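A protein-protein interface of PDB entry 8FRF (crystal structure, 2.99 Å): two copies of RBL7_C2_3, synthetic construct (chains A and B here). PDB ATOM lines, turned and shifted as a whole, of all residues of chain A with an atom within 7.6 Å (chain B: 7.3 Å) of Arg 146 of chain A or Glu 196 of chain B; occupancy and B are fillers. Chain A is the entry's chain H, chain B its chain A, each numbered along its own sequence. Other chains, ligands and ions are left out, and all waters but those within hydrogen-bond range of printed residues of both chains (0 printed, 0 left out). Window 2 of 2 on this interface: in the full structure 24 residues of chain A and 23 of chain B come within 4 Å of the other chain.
Positions printed for both chains: 188, 190, 191 and 194.
Of the 11 pairs that touch across the chains among the printed residues, none has its exchanged pair printed and touching as well.
NH2 of Arg 146 of chain A lies within salt-bridge range of OE1 of Glu 196 of chain B (3.3 Å).
Of the 18 printed residues of chain B, 5 touch a printed residue of chain A.
Printed residues of chain B that touch a printed residue of chain A: Leu 193, Glu 196, Val 197, Gln 200 and Leu 201.
Along chain B the printed residues that touch a printed residue of chain A span positions 193 to 201.
Of the 19 printed residues of chain A, 6 touch a printed residue of chain B.
Printed residues of chain A that touch a printed residue of chain B: Arg 146, Ala 150, Leu 151, Ser 154, Glu 190 and Leu 194.
Hydrophobic or aromatic side chains of chain A that line the printed part of chain B: Ala 150, Leu 151 and Leu 194.
Along chain A the printed residues that touch a printed residue of chain B span positions 146 to 194.
Among the printed residues, 11 pairs touch across the chains.
Among the printed residues, Asp or Glu carboxylates within 4 Å of a Lys or Arg side-chain nitrogen of the other chain: Arg 146 of chain A with Glu 196 of chain B (3.3 Å).
Arg 146 of chain A touches just these residues of chain B: Leu 193 and Glu 196.
Printed residues of chain B within 4 Å of Glu 190 of chain A: Leu 193 (3.6 Å).
Of the printed residues of chain A, Leu 193 of chain B touches Arg 146 (3.6 Å), Ala 150 (3.9 Å), Glu 190 (3.6 Å) and Leu 194 (3.7 Å).
Of the printed residues of chain A, Gln 200 of chain B touches Ala 150, Leu 151 and Ser 154.
Printed residues of chain A within 4 Å of Leu 201 of chain B: Ser 154 (3.6 Å).
The nearest printed residue of chain A that does not touch Leu 193 of chain B is Gln 149 of chain A (5.3 Å).
The side-chain amide nitrogen (NE2) of Gln 149 of chain A lies close to the backbone NH (N) of Arg 146 of chain A (3.2 Å).
The side-chain carboxylate of Glu 190 of chain A is in salt-bridge range of the guanidinium group of Arg 146 of chain A (2.6 Å).
The backbone carbonyl oxygen (O) of Leu 151 of chain A is in hydrogen-bond range of the side-chain hydroxyl (OG) of Ser 154 of chain A.
CD1 of Leu 193 of chain B touches CZ of Arg 146 of chain A, at 3.6 Å.
Leu 193 of chain B touches Ala 150 of chain A (CD1 to CB, 3.9 Å).
Ala 150 of chain A touches Val 197 of chain B (O to CG2, 3.9 Å).
Gln 200 of chain B touches Ala 150 of chain A.
Leu 151 of chain A touches Gln 200 of chain B.
O of Val 197 of chain B touches CB of Ser 154 of chain A (3.7 Å).
Gln 200 of chain B touches Ser 154 of chain A (CB to OG, 3.6 Å).
Leu 201 of chain B touches Ser 154 of chain A.
CD2 of Leu 193 of chain B touches CB of Glu 190 of chain A (3.6 Å).
CD2 of Leu 194 of chain A touches CD2 of Leu 193 of chain B (3.7 Å).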
ATOM      1  N   GLU A 103      31.891  17.901 -32.272  1.00  0.00           N
ATOM      2  CA  GLU A 103      30.581  17.258 -32.231  1.00  0.00           C
ATOM      3  C   GLU A 103      30.125  16.822 -33.618  1.00  0.00           C
ATOM      4  O   GLU A 103      29.436  15.804 -33.750  1.00  0.00           O
ATOM      5  CB  GLU A 103      29.552  18.189 -31.587  1.00  0.00           C
ATOM      6  CG  GLU A 103      29.754  18.373 -30.090  1.00  0.00           C
ATOM      7  CD  GLU A 103      28.676  19.225 -29.442  1.00  0.00           C
ATOM      8  OE1 GLU A 103      27.687  19.561 -30.129  1.00  0.00           O
ATOM      9  OE2 GLU A 103      28.820  19.555 -28.241  1.00  0.00           O
ATOM     10  N   GLN A 106      31.965  13.631 -34.364  1.00  0.00           N
ATOM     11  CA  GLN A 106      31.429  12.555 -33.540  1.00  0.00           C
ATOM     12  C   GLN A 106      30.232  11.903 -34.215  1.00  0.00           C
ATOM     13  O   GLN A 106      30.146  10.673 -34.308  1.00  0.00           O
ATOM     14  CB  GLN A 106      31.039  13.112 -32.172  1.00  0.00           C
ATOM     15  CG  GLN A 106      32.218  13.464 -31.298  1.00  0.00           C
ATOM     16  CD  GLN A 106      31.837  14.394 -30.162  1.00  0.00           C
ATOM     17  OE1 GLN A 106      30.728  14.327 -29.623  1.00  0.00           O
ATOM     18  NE2 GLN A 106      32.755  15.278 -29.801  1.00  0.00           N
ATOM     19  N   ILE A 140      36.439   6.965 -23.632  1.00  0.00           N
ATOM     20  CA  ILE A 140      35.610   8.071 -24.100  1.00  0.00           C
ATOM     21  C   ILE A 140      34.540   8.418 -23.075  1.00  0.00           C
ATOM     22  O   ILE A 140      34.204   9.592 -22.881  1.00  0.00           O
ATOM     23  CB  ILE A 140      34.997   7.728 -25.471  1.00  0.00           C
ATOM     24  CG1 ILE A 140      36.118   7.411 -26.467  1.00  0.00           C
ATOM     25  CG2 ILE A 140      34.082   8.862 -25.956  1.00  0.00           C
ATOM     26  CD1 ILE A 140      35.638   6.840 -27.780  1.00  0.00           C
ATOM     27  N   ILE A 141      33.977   7.406 -22.411  1.00  0.00           N
ATOM     28  CA  ILE A 141      32.981   7.672 -21.377  1.00  0.00           C
ATOM     29  C   ILE A 141      33.622   8.329 -20.156  1.00  0.00           C
ATOM     30  O   ILE A 141      33.059   9.261 -19.566  1.00  0.00           O
ATOM     31  CB  ILE A 141      32.251   6.364 -21.010  1.00  0.00           C
ATOM     32  CG1 ILE A 141      31.338   5.929 -22.159  1.00  0.00           C
ATOM     33  CG2 ILE A 141      31.448   6.536 -19.735  1.00  0.00           C
ATOM     34  CD1 ILE A 141      30.741   4.542 -22.000  1.00  0.00           C
ATOM     35  N   GLN A 143      36.454  10.166 -19.819  1.00  0.00           N
ATOM     36  CA  GLN A 143      37.113  11.459 -19.946  1.00  0.00           C
ATOM     37  C   GLN A 143      36.496  12.329 -21.029  1.00  0.00           C
ATOM     38  O   GLN A 143      37.034  13.404 -21.329  1.00  0.00           O
ATOM     39  CB  GLN A 143      38.608  11.268 -20.234  1.00  0.00           C
ATOM     40  CG  GLN A 143      39.440  10.803 -19.046  1.00  0.00           C
ATOM     41  CD  GLN A 143      40.865  10.429 -19.432  1.00  0.00           C
ATOM     42  OE1 GLN A 143      41.193  10.316 -20.615  1.00  0.00           O
ATOM     43  NE2 GLN A 143      41.722  10.252 -18.430  1.00  0.00           N
ATOM     44  N   GLY A 144      35.350  11.930 -21.577  1.00  0.00           N
ATOM     45  CA  GLY A 144      34.705  12.675 -22.631  1.00  0.00           C
ATOM     46  C   GLY A 144      33.602  13.588 -22.119  1.00  0.00           C
ATOM     47  O   GLY A 144      33.255  13.608 -20.941  1.00  0.00           O
ATOM     48  N   SER A 145      33.036  14.341 -23.058  1.00  0.00           N
ATOM     49  CA  SER A 145      31.938  15.250 -22.776  1.00  0.00           C
ATOM     50  C   SER A 145      30.647  14.478 -22.512  1.00  0.00           C
ATOM     51  O   SER A 145      30.566  13.257 -22.682  1.00  0.00           O
ATOM     52  CB  SER A 145      31.734  16.206 -23.947  1.00  0.00           C
ATOM     53  OG  SER A 145      31.474  15.474 -25.135  1.00  0.00           O
ATOM     54  N   ARG A 146      29.623  15.217 -22.077  1.00  0.00           N
ATOM     55  CA  ARG A 146      28.317  14.609 -21.857  1.00  0.00           C
ATOM     56  C   ARG A 146      27.743  14.064 -23.159  1.00  0.00           C
ATOM     57  O   ARG A 146      27.075  13.023 -23.154  1.00  0.00           O
ATOM     58  CB  ARG A 146      27.378  15.630 -21.201  1.00  0.00           C
ATOM     59  CG  ARG A 146      25.907  15.227 -21.112  1.00  0.00           C
ATOM     60  CD  ARG A 146      25.642  13.891 -20.425  1.00  0.00           C
ATOM     61  NE  ARG A 146      24.204  13.661 -20.320  1.00  0.00           N
ATOM     62  CZ  ARG A 146      23.449  13.175 -21.298  1.00  0.00           C
ATOM     63  NH1 ARG A 146      23.966  12.839 -22.470  1.00  0.00           N
ATOM     64  NH2 ARG A 146      22.138  13.049 -21.106  1.00  0.00           N
ATOM     65  N   GLU A 147      28.029  14.724 -24.286  1.00  0.00           N
ATOM     66  CA  GLU A 147      27.617  14.185 -25.577  1.00  0.00           C
ATOM     67  C   GLU A 147      28.387  12.917 -25.905  1.00  0.00           C
ATOM     68  O   GLU A 147      27.805  11.932 -26.374  1.00  0.00           O
ATOM     69  CB  GLU A 147      27.838  15.221 -26.680  1.00  0.00           C
ATOM     70  CG  GLU A 147      26.885  16.384 -26.659  1.00  0.00           C
ATOM     71  CD  GLU A 147      25.549  16.029 -27.269  1.00  0.00           C
ATOM     72  OE1 GLU A 147      25.413  16.150 -28.506  1.00  0.00           O
ATOM     73  OE2 GLU A 147      24.645  15.610 -26.515  1.00  0.00           O
ATOM     74  N   GLN A 148      29.694  12.914 -25.638  1.00  0.00           N
ATOM     75  CA  GLN A 148      30.503  11.739 -25.932  1.00  0.00           C
ATOM     76  C   GLN A 148      30.118  10.562 -25.044  1.00  0.00           C
ATOM     77  O   GLN A 148      30.101   9.413 -25.503  1.00  0.00           O
ATOM     78  CB  GLN A 148      31.980  12.089 -25.771  1.00  0.00           C
ATOM     79  CG  GLN A 148      32.515  12.940 -26.904  1.00  0.00           C
ATOM     80  CD  GLN A 148      33.948  13.357 -26.689  1.00  0.00           C
ATOM     81  OE1 GLN A 148      34.381  13.559 -25.558  1.00  0.00           O
ATOM     82  NE2 GLN A 148      34.700  13.487 -27.780  1.00  0.00           N
ATOM     83  N   GLN A 149      29.771  10.839 -23.782  1.00  0.00           N
ATOM     84  CA  GLN A 149      29.333   9.791 -22.864  1.00  0.00           C
ATOM     85  C   GLN A 149      28.171   8.994 -23.431  1.00  0.00           C
ATOM     86  O   GLN A 149      28.217   7.758 -23.487  1.00  0.00           O
ATOM     87  CB  GLN A 149      28.928  10.413 -21.532  1.00  0.00           C
ATOM     88  CG  GLN A 149      29.970  10.438 -20.445  1.00  0.00           C
ATOM     89  CD  GLN A 149      29.850  11.680 -19.608  1.00  0.00           C
ATOM     90  OE1 GLN A 149      29.410  11.643 -18.462  1.00  0.00           O
ATOM     91  NE2 GLN A 149      30.320  12.784 -20.150  1.00  0.00           N
ATOM     92  N   ALA A 150      27.110   9.684 -23.852  1.00  0.00           N
ATOM     93  CA  ALA A 150      25.942   8.978 -24.357  1.00  0.00           C
ATOM     94  C   ALA A 150      26.270   8.247 -25.650  1.00  0.00           C
ATOM     95  O   ALA A 150      25.894   7.080 -25.820  1.00  0.00           O
ATOM     96  CB  ALA A 150      24.786   9.956 -24.562  1.00  0.00           C
ATOM     97  N   LEU A 151      27.002   8.903 -26.555  1.00  0.00           N
ATOM     98  CA  LEU A 151      27.338   8.280 -27.832  1.00  0.00           C
ATOM     99  C   LEU A 151      28.243   7.075 -27.632  1.00  0.00           C
ATOM    100  O   LEU A 151      27.978   5.997 -28.174  1.00  0.00           O
ATOM    101  CB  LEU A 151      27.976   9.303 -28.772  1.00  0.00           C
ATOM    102  CG  LEU A 151      28.591   8.778 -30.071  1.00  0.00           C
ATOM    103  CD1 LEU A 151      27.594   7.970 -30.867  1.00  0.00           C
ATOM    104  CD2 LEU A 151      29.059   9.971 -30.897  1.00  0.00           C
ATOM    105  N   ALA A 152      29.326   7.239 -26.866  1.00  0.00           N
ATOM    106  CA  ALA A 152      30.191   6.099 -26.595  1.00  0.00           C
ATOM    107  C   ALA A 152      29.434   4.986 -25.887  1.00  0.00           C
ATOM    108  O   ALA A 152      29.727   3.803 -26.098  1.00  0.00           O
ATOM    109  CB  ALA A 152      31.395   6.528 -25.764  1.00  0.00           C
ATOM    110  N   SER A 154      26.146   4.132 -26.323  1.00  0.00           N
ATOM    111  CA  SER A 154      25.339   3.379 -27.275  1.00  0.00           C
ATOM    112  C   SER A 154      26.208   2.591 -28.245  1.00  0.00           C
ATOM    113  O   SER A 154      25.877   1.450 -28.589  1.00  0.00           O
ATOM    114  CB  SER A 154      24.398   4.323 -28.028  1.00  0.00           C
ATOM    115  OG  SER A 154      25.115   5.249 -28.821  1.00  0.00           O
ATOM    116  N   SER A 188      31.190  11.598 -12.854  1.00  0.00           N
ATOM    117  CA  SER A 188      30.032  12.431 -12.571  1.00  0.00           C
ATOM    118  C   SER A 188      28.834  11.564 -12.191  1.00  0.00           C
ATOM    119  O   SER A 188      28.892  10.331 -12.207  1.00  0.00           O
ATOM    120  CB  SER A 188      29.701  13.301 -13.780  1.00  0.00           C
ATOM    121  OG  SER A 188      29.332  12.499 -14.892  1.00  0.00           O
ATOM    122  N   GLU A 190      26.193  11.171 -13.924  1.00  0.00           N
ATOM    123  CA  GLU A 190      25.822  10.435 -15.125  1.00  0.00           C
ATOM    124  C   GLU A 190      26.868   9.390 -15.485  1.00  0.00           C
ATOM    125  O   GLU A 190      26.523   8.291 -15.938  1.00  0.00           O
ATOM    126  CB  GLU A 190      25.599  11.417 -16.275  1.00  0.00           C
ATOM    127  CG  GLU A 190      24.291  12.192 -16.159  1.00  0.00           C
ATOM    128  CD  GLU A 190      24.343  13.532 -16.867  1.00  0.00           C
ATOM    129  OE1 GLU A 190      25.194  14.360 -16.483  1.00  0.00           O
ATOM    130  OE2 GLU A 190      23.550  13.752 -17.809  1.00  0.00           O
ATOM    131  N   GLN A 191      28.148   9.712 -15.301  1.00  0.00           N
ATOM    132  CA  GLN A 191      29.189   8.724 -15.564  1.00  0.00           C
ATOM    133  C   GLN A 191      29.060   7.522 -14.638  1.00  0.00           C
ATOM    134  O   GLN A 191      29.138   6.373 -15.086  1.00  0.00           O
ATOM    135  CB  GLN A 191      30.562   9.374 -15.412  1.00  0.00           C
ATOM    136  CG  GLN A 191      31.008  10.050 -16.668  1.00  0.00           C
ATOM    137  CD  GLN A 191      32.219  10.908 -16.483  1.00  0.00           C
ATOM    138  OE1 GLN A 191      32.422  11.503 -15.426  1.00  0.00           O
ATOM    139  NE2 GLN A 191      33.036  10.994 -17.525  1.00  0.00           N
ATOM    140  N   LEU A 194      26.228   5.308 -15.828  1.00  0.00           N
ATOM    141  CA  LEU A 194      26.641   4.479 -16.957  1.00  0.00           C
ATOM    142  C   LEU A 194      27.554   3.355 -16.498  1.00  0.00           C
ATOM    143  O   LEU A 194      27.440   2.221 -16.974  1.00  0.00           O
ATOM    144  CB  LEU A 194      27.349   5.323 -18.018  1.00  0.00           C
ATOM    145  CG  LEU A 194      26.541   6.354 -18.808  1.00  0.00           C
ATOM    146  CD1 LEU A 194      27.409   6.974 -19.895  1.00  0.00           C
ATOM    147  CD2 LEU A 194      25.277   5.743 -19.399  1.00  0.00           C
ATOM    148  N   LEU B 180      10.373   5.395 -24.609  1.00  0.00           N
ATOM    149  CA  LEU B 180      11.663   6.033 -24.355  1.00  0.00           C
ATOM    150  C   LEU B 180      11.596   7.538 -24.571  1.00  0.00           C
ATOM    151  O   LEU B 180      12.230   8.304 -23.836  1.00  0.00           O
ATOM    152  CB  LEU B 180      12.730   5.430 -25.264  1.00  0.00           C
ATOM    153  CG  LEU B 180      13.343   4.103 -24.843  1.00  0.00           C
ATOM    154  CD1 LEU B 180      14.129   3.535 -26.016  1.00  0.00           C
ATOM    155  CD2 LEU B 180      14.237   4.308 -23.628  1.00  0.00           C
ATOM    156  N   ILE B 183      10.133   8.973 -21.488  1.00  0.00           N
ATOM    157  CA  ILE B 183      11.131   9.040 -20.421  1.00  0.00           C
ATOM    158  C   ILE B 183      12.048  10.237 -20.629  1.00  0.00           C
ATOM    159  O   ILE B 183      12.450  10.906 -19.671  1.00  0.00           O
ATOM    160  CB  ILE B 183      11.925   7.722 -20.343  1.00  0.00           C
ATOM    161  CG1 ILE B 183      10.981   6.548 -20.067  1.00  0.00           C
ATOM    162  CG2 ILE B 183      13.014   7.812 -19.281  1.00  0.00           C
ATOM    163  CD1 ILE B 183      11.634   5.191 -20.148  1.00  0.00           C
ATOM    164  N   GLN B 184      12.378  10.537 -21.886  1.00  0.00           N
ATOM    165  CA  GLN B 184      13.275  11.651 -22.169  1.00  0.00           C
ATOM    166  C   GLN B 184      12.626  13.002 -21.915  1.00  0.00           C
ATOM    167  O   GLN B 184      13.310  13.941 -21.497  1.00  0.00           O
ATOM    168  CB  GLN B 184      13.756  11.581 -23.613  1.00  0.00           C
ATOM    169  CG  GLN B 184      14.742  12.660 -23.982  1.00  0.00           C
ATOM    170  CD  GLN B 184      15.068  12.656 -25.455  1.00  0.00           C
ATOM    171  OE1 GLN B 184      15.586  11.673 -25.977  1.00  0.00           O
ATOM    172  NE2 GLN B 184      14.722  13.738 -26.145  1.00  0.00           N
ATOM    173  N   SER B 188      14.227  12.439 -15.130  1.00  0.00           N
ATOM    174  CA  SER B 188      15.340  13.080 -14.442  1.00  0.00           C
ATOM    175  C   SER B 188      16.547  13.196 -15.376  1.00  0.00           C
ATOM    176  O   SER B 188      16.540  12.713 -16.513  1.00  0.00           O
ATOM    177  CB  SER B 188      15.711  12.299 -13.184  1.00  0.00           C
ATOM    178  OG  SER B 188      16.184  10.998 -13.500  1.00  0.00           O
ATOM    179  N   ASP B 189      17.610  13.840 -14.884  1.00  0.00           N
ATOM    180  CA  ASP B 189      18.823  13.950 -15.691  1.00  0.00           C
ATOM    181  C   ASP B 189      19.404  12.577 -15.996  1.00  0.00           C
ATOM    182  O   ASP B 189      19.860  12.326 -17.119  1.00  0.00           O
ATOM    183  CB  ASP B 189      19.868  14.826 -14.988  1.00  0.00           C
ATOM    184  CG  ASP B 189      19.552  16.314 -15.074  1.00  0.00           C
ATOM    185  OD1 ASP B 189      18.390  16.668 -15.376  1.00  0.00           O
ATOM    186  OD2 ASP B 189      20.470  17.135 -14.856  1.00  0.00           O
ATOM    187  N   GLU B 190      19.348  11.660 -15.025  1.00  0.00           N
ATOM    188  CA  GLU B 190      19.865  10.315 -15.251  1.00  0.00           C
ATOM    189  C   GLU B 190      18.921   9.479 -16.103  1.00  0.00           C
ATOM    190  O   GLU B 190      19.376   8.716 -16.964  1.00  0.00           O
ATOM    191  CB  GLU B 190      20.139   9.623 -13.917  1.00  0.00           C
ATOM    192  CG  GLU B 190      21.399  10.112 -13.220  1.00  0.00           C
ATOM    193  CD  GLU B 190      21.372   9.882 -11.720  1.00  0.00           C
ATOM    194  OE1 GLU B 190      20.471  10.429 -11.042  1.00  0.00           O
ATOM    195  OE2 GLU B 190      22.248   9.142 -11.223  1.00  0.00           O
ATOM    196  N   GLN B 191      17.609   9.607 -15.879  1.00  0.00           N
ATOM    197  CA  GLN B 191      16.644   8.905 -16.720  1.00  0.00           C
ATOM    198  C   GLN B 191      16.737   9.364 -18.167  1.00  0.00           C
ATOM    199  O   GLN B 191      16.667   8.542 -19.090  1.00  0.00           O
ATOM    200  CB  GLN B 191      15.230   9.112 -16.185  1.00  0.00           C
ATOM    201  CG  GLN B 191      14.834   8.107 -15.140  1.00  0.00           C
ATOM    202  CD  GLN B 191      13.548   8.464 -14.430  1.00  0.00           C
ATOM    203  OE1 GLN B 191      13.245   9.640 -14.216  1.00  0.00           O
ATOM    204  NE2 GLN B 191      12.781   7.447 -14.057  1.00  0.00           N
ATOM    205  N   ARG B 192      16.904  10.673 -18.389  1.00  0.00           N
ATOM    206  CA  ARG B 192      17.012  11.172 -19.757  1.00  0.00           C
ATOM    207  C   ARG B 192      18.252  10.620 -20.442  1.00  0.00           C
ATOM    208  O   ARG B 192      18.221  10.312 -21.639  1.00  0.00           O
ATOM    209  CB  ARG B 192      17.013  12.697 -19.780  1.00  0.00           C
ATOM    210  CG  ARG B 192      15.647  13.284 -19.479  1.00  0.00           C
ATOM    211  CD  ARG B 192      15.652  14.784 -19.620  1.00  0.00           C
ATOM    212  NE  ARG B 192      16.388  15.436 -18.545  1.00  0.00           N
ATOM    213  CZ  ARG B 192      17.564  16.020 -18.708  1.00  0.00           C
ATOM    214  NH1 ARG B 192      18.188  16.005 -19.877  1.00  0.00           N
ATOM    215  NH2 ARG B 192      18.122  16.649 -17.680  1.00  0.00           N
ATOM    216  N   LEU B 193      19.352  10.481 -19.700  1.00  0.00           N
ATOM    217  CA  LEU B 193      20.560   9.900 -20.273  1.00  0.00           C
ATOM    218  C   LEU B 193      20.330   8.459 -20.711  1.00  0.00           C
ATOM    219  O   LEU B 193      20.701   8.072 -21.825  1.00  0.00           O
ATOM    220  CB  LEU B 193      21.707   9.981 -19.270  1.00  0.00           C
ATOM    221  CG  LEU B 193      22.915   9.112 -19.617  1.00  0.00           C
ATOM    222  CD1 LEU B 193      23.633   9.651 -20.839  1.00  0.00           C
ATOM    223  CD2 LEU B 193      23.861   9.045 -18.432  1.00  0.00           C
ATOM    224  N   LEU B 194      19.721   7.645 -19.842  1.00  0.00           N
ATOM    225  CA  LEU B 194      19.429   6.260 -20.203  1.00  0.00           C
ATOM    226  C   LEU B 194      18.520   6.193 -21.424  1.00  0.00           C
ATOM    227  O   LEU B 194      18.708   5.347 -22.306  1.00  0.00           O
ATOM    228  CB  LEU B 194      18.773   5.541 -19.024  1.00  0.00           C
ATOM    229  CG  LEU B 194      19.584   5.275 -17.753  1.00  0.00           C
ATOM    230  CD1 LEU B 194      18.763   4.456 -16.766  1.00  0.00           C
ATOM    231  CD2 LEU B 194      20.896   4.583 -18.065  1.00  0.00           C
ATOM    232  N   ALA B 195      17.537   7.090 -21.498  1.00  0.00           N
ATOM    233  CA  ALA B 195      16.630   7.106 -22.638  1.00  0.00           C
ATOM    234  C   ALA B 195      17.358   7.497 -23.916  1.00  0.00           C
ATOM    235  O   ALA B 195      17.170   6.865 -24.962  1.00  0.00           O
ATOM    236  CB  ALA B 195      15.468   8.061 -22.358  1.00  0.00           C
ATOM    237  N   GLU B 196      18.201   8.530 -23.845  1.00  0.00           N
ATOM    238  CA  GLU B 196      18.957   8.971 -25.015  1.00  0.00           C
ATOM    239  C   GLU B 196      19.919   7.890 -25.496  1.00  0.00           C
ATOM    240  O   GLU B 196      20.125   7.722 -26.703  1.00  0.00           O
ATOM    241  CB  GLU B 196      19.715  10.254 -24.677  1.00  0.00           C
ATOM    242  CG  GLU B 196      18.816  11.462 -24.475  1.00  0.00           C
ATOM    243  CD  GLU B 196      19.569  12.676 -23.969  1.00  0.00           C
ATOM    244  OE1 GLU B 196      20.814  12.690 -24.087  1.00  0.00           O
ATOM    245  OE2 GLU B 196      18.916  13.613 -23.454  1.00  0.00           O
ATOM    246  N   VAL B 197      20.502   7.133 -24.565  1.00  0.00           N
ATOM    247  CA  VAL B 197      21.376   6.031 -24.952  1.00  0.00           C
ATOM    248  C   VAL B 197      20.585   4.983 -25.723  1.00  0.00           C
ATOM    249  O   VAL B 197      20.952   4.596 -26.839  1.00  0.00           O
ATOM    250  CB  VAL B 197      22.054   5.425 -23.709  1.00  0.00           C
ATOM    251  CG1 VAL B 197      22.671   4.074 -24.042  1.00  0.00           C
ATOM    252  CG2 VAL B 197      23.098   6.374 -23.167  1.00  0.00           C
ATOM    253  N   LEU B 198      19.465   4.537 -25.153  1.00  0.00           N
ATOM    254  CA  LEU B 198      18.668   3.510 -25.807  1.00  0.00           C
ATOM    255  C   LEU B 198      18.091   4.017 -27.120  1.00  0.00           C
ATOM    256  O   LEU B 198      17.962   3.249 -28.081  1.00  0.00           O
ATOM    257  CB  LEU B 198      17.557   3.036 -24.869  1.00  0.00           C
ATOM    258  CG  LEU B 198      18.056   2.256 -23.648  1.00  0.00           C
ATOM    259  CD1 LEU B 198      16.919   1.925 -22.686  1.00  0.00           C
ATOM    260  CD2 LEU B 198      18.788   0.994 -24.086  1.00  0.00           C
ATOM    261  N   LEU B 199      17.750   5.305 -27.185  1.00  0.00           N
ATOM    262  CA  LEU B 199      17.258   5.867 -28.436  1.00  0.00           C
ATOM    263  C   LEU B 199      18.341   5.864 -29.513  1.00  0.00           C
ATOM    264  O   LEU B 199      18.062   5.534 -30.671  1.00  0.00           O
ATOM    265  CB  LEU B 199      16.720   7.277 -28.199  1.00  0.00           C
ATOM    266  CG  LEU B 199      15.343   7.348 -27.528  1.00  0.00           C
ATOM    267  CD1 LEU B 199      15.027   8.768 -27.101  1.00  0.00           C
ATOM    268  CD2 LEU B 199      14.252   6.804 -28.426  1.00  0.00           C
ATOM    269  N   GLN B 200      19.584   6.199 -29.156  1.00  0.00           N
ATOM    270  CA  GLN B 200      20.663   6.155 -30.142  1.00  0.00           C
ATOM    271  C   GLN B 200      20.964   4.728 -30.573  1.00  0.00           C
ATOM    272  O   GLN B 200      21.232   4.476 -31.753  1.00  0.00           O
ATOM    273  CB  GLN B 200      21.930   6.799 -29.584  1.00  0.00           C
ATOM    274  CG  GLN B 200      21.879   8.306 -29.422  1.00  0.00           C
ATOM    275  CD  GLN B 200      23.241   8.889 -29.069  1.00  0.00           C
ATOM    276  OE1 GLN B 200      23.447   9.369 -27.951  1.00  0.00           O
ATOM    277  NE2 GLN B 200      24.182   8.835 -30.009  1.00  0.00           N
ATOM    278  N   LEU B 201      20.942   3.783 -29.631  1.00  0.00           N
ATOM    279  CA  LEU B 201      21.211   2.395 -29.983  1.00  0.00           C
ATOM    280  C   LEU B 201      20.178   1.865 -30.968  1.00  0.00           C
ATOM    281  O   LEU B 201      20.534   1.209 -31.956  1.00  0.00           O
ATOM    282  CB  LEU B 201      21.249   1.527 -28.727  1.00  0.00           C
ATOM    283  CG  LEU B 201      21.482   0.030 -28.939  1.00  0.00           C
ATOM    284  CD1 LEU B 201      22.809  -0.221 -29.641  1.00  0.00           C
ATOM    285  CD2 LEU B 201      21.435  -0.686 -27.599  1.00  0.00           C
ATOM    286  N   LEU B 202      18.896   2.155 -30.728  1.00  0.00           N
ATOM    287  CA  LEU B 202      17.851   1.674 -31.626  1.00  0.00           C
ATOM    288  C   LEU B 202      17.988   2.271 -33.020  1.00  0.00           C
ATOM    289  O   LEU B 202      17.853   1.559 -34.024  1.00  0.00           O
ATOM    290  CB  LEU B 202      16.469   1.992 -31.051  1.00  0.00           C
ATOM    291  CG  LEU B 202      15.748   0.917 -30.235  1.00  0.00           C
ATOM    292  CD1 LEU B 202      16.587   0.448 -29.052  1.00  0.00           C
ATOM    293  CD2 LEU B 202      14.410   1.448 -29.764  1.00  0.00           C
